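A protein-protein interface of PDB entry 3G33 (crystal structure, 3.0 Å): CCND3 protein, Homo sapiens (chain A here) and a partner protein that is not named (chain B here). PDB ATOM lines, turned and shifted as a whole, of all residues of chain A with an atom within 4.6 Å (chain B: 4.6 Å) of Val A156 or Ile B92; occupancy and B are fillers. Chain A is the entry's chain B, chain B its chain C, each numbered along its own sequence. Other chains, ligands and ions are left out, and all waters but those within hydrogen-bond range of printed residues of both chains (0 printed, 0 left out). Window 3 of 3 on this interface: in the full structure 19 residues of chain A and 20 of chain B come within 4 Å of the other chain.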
ATOM      1  N   ARG A 152      11.067 -13.697  16.265  1.00  0.00           N
ATOM      2  CA  ARG A 152      10.543 -15.041  16.478  1.00  0.00           C
ATOM      3  C   ARG A 152      11.434 -15.816  17.441  1.00  0.00           C
ATOM      4  O   ARG A 152      10.951 -16.429  18.393  1.00  0.00           O
ATOM      5  CB  ARG A 152      10.437 -15.787  15.150  1.00  0.00           C
ATOM      6  CG  ARG A 152       9.623 -15.057  14.099  1.00  0.00           C
ATOM      7  CD  ARG A 152       9.916 -15.594  12.711  1.00  0.00           C
ATOM      8  NE  ARG A 152       9.390 -14.718  11.668  1.00  0.00           N
ATOM      9  CZ  ARG A 152       9.751 -14.778  10.390  1.00  0.00           C
ATOM     10  NH1 ARG A 152      10.646 -15.673   9.994  1.00  0.00           N
ATOM     11  NH2 ARG A 152       9.221 -13.942   9.509  1.00  0.00           N
ATOM     12  N   ASP A 153      12.737 -15.782  17.185  1.00  0.00           N
ATOM     13  CA  ASP A 153      13.707 -16.485  18.015  1.00  0.00           C
ATOM     14  C   ASP A 153      13.704 -15.967  19.449  1.00  0.00           C
ATOM     15  O   ASP A 153      13.627 -16.746  20.399  1.00  0.00           O
ATOM     16  CB  ASP A 153      15.111 -16.355  17.420  1.00  0.00           C
ATOM     17  CG  ASP A 153      15.254 -17.084  16.100  1.00  0.00           C
ATOM     18  OD1 ASP A 153      14.811 -18.249  16.013  1.00  0.00           O
ATOM     19  OD2 ASP A 153      15.813 -16.496  15.151  1.00  0.00           O
ATOM     20  N   TRP A 154      13.791 -14.650  19.599  1.00  0.00           N
ATOM     21  CA  TRP A 154      13.878 -14.037  20.921  1.00  0.00           C
ATOM     22  C   TRP A 154      12.601 -14.194  21.737  1.00  0.00           C
ATOM     23  O   TRP A 154      12.635 -14.138  22.967  1.00  0.00           O
ATOM     24  CB  TRP A 154      14.274 -12.564  20.810  1.00  0.00           C
ATOM     25  CG  TRP A 154      15.754 -12.362  20.746  1.00  0.00           C
ATOM     26  CD1 TRP A 154      16.577 -12.656  19.698  1.00  0.00           C
ATOM     27  CD2 TRP A 154      16.592 -11.828  21.777  1.00  0.00           C
ATOM     28  NE1 TRP A 154      17.876 -12.336  20.012  1.00  0.00           N
ATOM     29  CE2 TRP A 154      17.912 -11.825  21.282  1.00  0.00           C
ATOM     30  CE3 TRP A 154      16.355 -11.349  23.069  1.00  0.00           C
ATOM     31  CZ2 TRP A 154      18.989 -11.363  22.036  1.00  0.00           C
ATOM     32  CZ3 TRP A 154      17.426 -10.890  23.815  1.00  0.00           C
ATOM     33  CH2 TRP A 154      18.726 -10.901  23.296  1.00  0.00           C
ATOM     34  N   GLU A 155      11.476 -14.390  21.057  1.00  0.00           N
ATOM     35  CA  GLU A 155      10.223 -14.655  21.749  1.00  0.00           C
ATOM     36  C   GLU A 155      10.343 -15.971  22.503  1.00  0.00           C
ATOM     37  O   GLU A 155       9.907 -16.089  23.648  1.00  0.00           O
ATOM     38  CB  GLU A 155       9.058 -14.724  20.762  1.00  0.00           C
ATOM     39  CG  GLU A 155       7.697 -14.850  21.429  1.00  0.00           C
ATOM     40  CD  GLU A 155       6.606 -15.257  20.458  1.00  0.00           C
ATOM     41  OE1 GLU A 155       6.927 -15.902  19.438  1.00  0.00           O
ATOM     42  OE2 GLU A 155       5.427 -14.937  20.717  1.00  0.00           O
ATOM     43  N   VAL A 156      10.943 -16.959  21.848  1.00  0.00           N
ATOM     44  CA  VAL A 156      11.166 -18.263  22.456  1.00  0.00           C
ATOM     45  C   VAL A 156      12.235 -18.169  23.537  1.00  0.00           C
ATOM     46  O   VAL A 156      12.174 -18.869  24.546  1.00  0.00           O
ATOM     47  CB  VAL A 156      11.605 -19.303  21.407  1.00  0.00           C
ATOM     48  CG1 VAL A 156      11.800 -20.664  22.058  1.00  0.00           C
ATOM     49  CG2 VAL A 156      10.585 -19.384  20.283  1.00  0.00           C
ATOM     50  N   LEU A 157      13.212 -17.296  23.318  1.00  0.00           N
ATOM     51  CA  LEU A 157      14.307 -17.114  24.261  1.00  0.00           C
ATOM     52  C   LEU A 157      13.809 -16.519  25.572  1.00  0.00           C
ATOM     53  O   LEU A 157      14.141 -17.005  26.652  1.00  0.00           O
ATOM     54  CB  LEU A 157      15.389 -16.218  23.655  1.00  0.00           C
ATOM     55  CG  LEU A 157      16.668 -16.044  24.477  1.00  0.00           C
ATOM     56  CD1 LEU A 157      17.365 -17.381  24.683  1.00  0.00           C
ATOM     57  CD2 LEU A 157      17.603 -15.046  23.809  1.00  0.00           C
ATOM     58  N   VAL A 158      13.010 -15.464  25.471  1.00  0.00           N
ATOM     59  CA  VAL A 158      12.482 -14.787  26.649  1.00  0.00           C
ATOM     60  C   VAL A 158      11.520 -15.680  27.425  1.00  0.00           C
ATOM     61  O   VAL A 158      11.539 -15.704  28.656  1.00  0.00           O
ATOM     62  CB  VAL A 158      11.767 -13.478  26.273  1.00  0.00           C
ATOM     63  CG1 VAL A 158      11.126 -12.857  27.501  1.00  0.00           C
ATOM     64  CG2 VAL A 158      12.745 -12.509  25.627  1.00  0.00           C
ATOM     65  N   LEU A 159      10.678 -16.411  26.702  1.00  0.00           N
ATOM     66  CA  LEU A 159       9.732 -17.330  27.326  1.00  0.00           C
ATOM     67  C   LEU A 159      10.448 -18.354  28.198  1.00  0.00           C
ATOM     68  O   LEU A 159      10.059 -18.591  29.342  1.00  0.00           O
ATOM     69  CB  LEU A 159       8.897 -18.046  26.263  1.00  0.00           C
ATOM     70  CG  LEU A 159       7.649 -17.320  25.763  1.00  0.00           C
ATOM     71  CD1 LEU A 159       7.123 -17.973  24.495  1.00  0.00           C
ATOM     72  CD2 LEU A 159       6.580 -17.294  26.844  1.00  0.00           C
ATOM     73  N   GLY A 160      11.493 -18.963  27.648  1.00  0.00           N
ATOM     74  CA  GLY A 160      12.261 -19.967  28.369  1.00  0.00           C
ATOM     75  C   GLY A 160      12.923 -19.409  29.611  1.00  0.00           C
ATOM     76  O   GLY A 160      12.950 -20.059  30.656  1.00  0.00           O
ATOM     77  N   VAL B  42       5.518 -31.218  23.089  1.00  0.00           N
ATOM     78  CA  VAL B  42       4.567 -30.898  22.032  1.00  0.00           C
ATOM     79  C   VAL B  42       5.264 -30.012  21.006  1.00  0.00           C
ATOM     80  O   VAL B  42       6.088 -29.175  21.368  1.00  0.00           O
ATOM     81  CB  VAL B  42       3.340 -30.147  22.579  1.00  0.00           C
ATOM     82  CG1 VAL B  42       2.515 -31.055  23.475  1.00  0.00           C
ATOM     83  CG2 VAL B  42       3.773 -28.896  23.328  1.00  0.00           C
ATOM     84  N   ARG B  43       4.947 -30.196  19.728  1.00  0.00           N
ATOM     85  CA  ARG B  43       5.530 -29.351  18.685  1.00  0.00           C
ATOM     86  C   ARG B  43       4.605 -28.183  18.322  1.00  0.00           C
ATOM     87  O   ARG B  43       3.450 -28.391  17.954  1.00  0.00           O
ATOM     88  CB  ARG B  43       5.910 -30.173  17.443  1.00  0.00           C
ATOM     89  CG  ARG B  43       4.826 -31.100  16.901  1.00  0.00           C
ATOM     90  CD  ARG B  43       5.333 -31.840  15.663  1.00  0.00           C
ATOM     91  NE  ARG B  43       4.329 -32.715  15.058  1.00  0.00           N
ATOM     92  CZ  ARG B  43       4.240 -34.022  15.285  1.00  0.00           C
ATOM     93  NH1 ARG B  43       5.092 -34.614  16.112  1.00  0.00           N
ATOM     94  NH2 ARG B  43       3.295 -34.738  14.689  1.00  0.00           N
ATOM     95  N   VAL B  44       5.116 -26.955  18.426  1.00  0.00           N
ATOM     96  CA  VAL B  44       4.288 -25.752  18.260  1.00  0.00           C
ATOM     97  C   VAL B  44       4.589 -24.952  16.989  1.00  0.00           C
ATOM     98  O   VAL B  44       5.540 -25.257  16.268  1.00  0.00           O
ATOM     99  CB  VAL B  44       4.439 -24.804  19.467  1.00  0.00           C
ATOM    100  CG1 VAL B  44       3.634 -23.533  19.246  1.00  0.00           C
ATOM    101  CG2 VAL B  44       4.005 -25.500  20.747  1.00  0.00           C
ATOM    102  N   ASN B  46       6.097 -21.919  14.988  1.00  0.00           N
ATOM    103  CA  ASN B  46       7.207 -20.983  15.169  1.00  0.00           C
ATOM    104  C   ASN B  46       7.214 -19.856  14.140  1.00  0.00           C
ATOM    105  O   ASN B  46       7.730 -18.770  14.400  1.00  0.00           O
ATOM    106  CB  ASN B  46       8.552 -21.717  15.148  1.00  0.00           C
ATOM    107  CG  ASN B  46       9.723 -20.797  15.451  1.00  0.00           C
ATOM    108  OD1 ASN B  46       9.540 -19.616  15.746  1.00  0.00           O
ATOM    109  ND2 ASN B  46      10.936 -21.338  15.381  1.00  0.00           N
ATOM    110  N   ALA B  84      12.143 -25.010  25.505  1.00  0.00           N
ATOM    111  CA  ALA B  84      11.808 -24.807  24.103  1.00  0.00           C
ATOM    112  C   ALA B  84      13.046 -24.910  23.219  1.00  0.00           C
ATOM    113  O   ALA B  84      14.090 -24.335  23.525  1.00  0.00           O
ATOM    114  CB  ALA B  84      11.132 -23.461  23.911  1.00  0.00           C
ATOM    115  N   THR B  85      12.920 -25.649  22.124  1.00  0.00           N
ATOM    116  CA  THR B  85      14.018 -25.813  21.182  1.00  0.00           C
ATOM    117  C   THR B  85      13.501 -25.777  19.750  1.00  0.00           C
ATOM    118  O   THR B  85      12.575 -26.506  19.397  1.00  0.00           O
ATOM    119  CB  THR B  85      14.767 -27.140  21.412  1.00  0.00           C
ATOM    120  OG1 THR B  85      15.125 -27.256  22.793  1.00  0.00           O
ATOM    121  CG2 THR B  85      16.024 -27.198  20.557  1.00  0.00           C
ATOM    122  N   SER B  86      14.101 -24.921  18.932  1.00  0.00           N
ATOM    123  CA  SER B  86      13.713 -24.806  17.532  1.00  0.00           C
ATOM    124  C   SER B  86      14.420 -25.859  16.685  1.00  0.00           C
ATOM    125  O   SER B  86      15.348 -25.547  15.940  1.00  0.00           O
ATOM    126  CB  SER B  86      14.031 -23.406  17.003  1.00  0.00           C
ATOM    127  OG  SER B  86      15.402 -23.094  17.183  1.00  0.00           O
ATOM    128  N   GLU B  91       8.613 -24.953  12.805  1.00  0.00           N
ATOM    129  CA  GLU B  91       7.955 -25.094  14.099  1.00  0.00           C
ATOM    130  C   GLU B  91       8.955 -25.200  15.246  1.00  0.00           C
ATOM    131  O   GLU B  91      10.167 -25.129  15.037  1.00  0.00           O
ATOM    132  CB  GLU B  91       7.019 -26.304  14.097  1.00  0.00           C
ATOM    133  CG  GLU B  91       7.676 -27.603  13.658  1.00  0.00           C
ATOM    134  CD  GLU B  91       6.680 -28.737  13.513  1.00  0.00           C
ATOM    135  OE1 GLU B  91       5.511 -28.559  13.916  1.00  0.00           O
ATOM    136  OE2 GLU B  91       7.064 -29.806  12.993  1.00  0.00           O
ATOM    137  N   ILE B  92       8.438 -25.370  16.459  1.00  0.00           N
ATOM    138  CA  ILE B  92       9.276 -25.422  17.649  1.00  0.00           C
ATOM    139  C   ILE B  92       8.731 -26.445  18.642  1.00  0.00           C
ATOM    140  O   ILE B  92       7.519 -26.585  18.797  1.00  0.00           O
ATOM    141  CB  ILE B  92       9.359 -24.040  18.325  1.00  0.00           C
ATOM    142  CG1 ILE B  92      10.709 -23.860  19.025  1.00  0.00           C
ATOM    143  CG2 ILE B  92       8.195 -23.843  19.289  1.00  0.00           C
ATOM    144  CD1 ILE B  92      10.994 -22.432  19.437  1.00  0.00           C
ATOM    145  N   LYS B  93       9.631 -27.161  19.308  1.00  0.00           N
ATOM    146  CA  LYS B  93       9.229 -28.192  20.259  1.00  0.00           C
ATOM    147  C   LYS B  93       9.267 -27.688  21.697  1.00  0.00           C
ATOM    148  O   LYS B  93      10.321 -27.315  22.212  1.00  0.00           O
ATOM    149  CB  LYS B  93      10.094 -29.445  20.099  1.00  0.00           C
ATOM    150  CG  LYS B  93       9.767 -30.246  18.849  1.00  0.00           C
ATOM    151  CD  LYS B  93      10.812 -31.309  18.560  1.00  0.00           C
ATOM    152  CE  LYS B  93      10.517 -32.013  17.245  1.00  0.00           C
ATOM    153  NZ  LYS B  93      10.340 -31.042  16.127  1.00  0.00           N
ATOM    154  N   VAL B  94       8.102 -27.680  22.335  1.00  0.00           N
ATOM    155  CA  VAL B  94       7.975 -27.206  23.704  1.00  0.00           C
ATOM    156  C   VAL B  94       7.895 -28.373  24.679  1.00  0.00           C
ATOM    157  O   VAL B  94       7.009 -29.222  24.573  1.00  0.00           O
ATOM    158  CB  VAL B  94       6.723 -26.331  23.878  1.00  0.00           C
ATOM    159  CG1 VAL B  94       6.576 -25.897  25.328  1.00  0.00           C
ATOM    160  CG2 VAL B  94       6.788 -25.126  22.951  1.00  0.00           C
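Among the printed residues, pairs that only touch across the chains: Arg A152 with Asn B46, Val A156 with Ala B84 and Val A156 with Ile B92.
N of Val B44 is in hydrogen-bond range of O of Ile B92 (2.5 Å).
Of the 9 printed residues of chain A, 2 touch a printed residue of chain B.
Hydrophobic or aromatic side chains of chain A within 4 Å of the printed part of chain B: Val A156.
Along chain A the printed residues that touch a printed residue of chain B span positions 152 to 156.
Hydrophobic or aromatic side chains of chain B within 4 Å of the printed part of chain A: Ala B84 and Ile B92.
Val A156 touches just these residues of chain B: Ala B84 and Ile B92.
Of the printed residues of chain A, Asn B46 touches Arg A152.
Of the printed residues of chain A, Ala B84 touches Val A156.
Ile B92 touches just one residue of chain A: Val A156 (3.2 Å).
The nearest printed residue of chain B that does not touch Val A156 is Asn B46 (4.7 Å).
The nearest printed residue of chain A that does not touch Ile B92 is Arg A152 (6.1 Å).
The nearest printed residue of chain B that does not touch Arg A152 is Ile B92 (6.1 Å).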
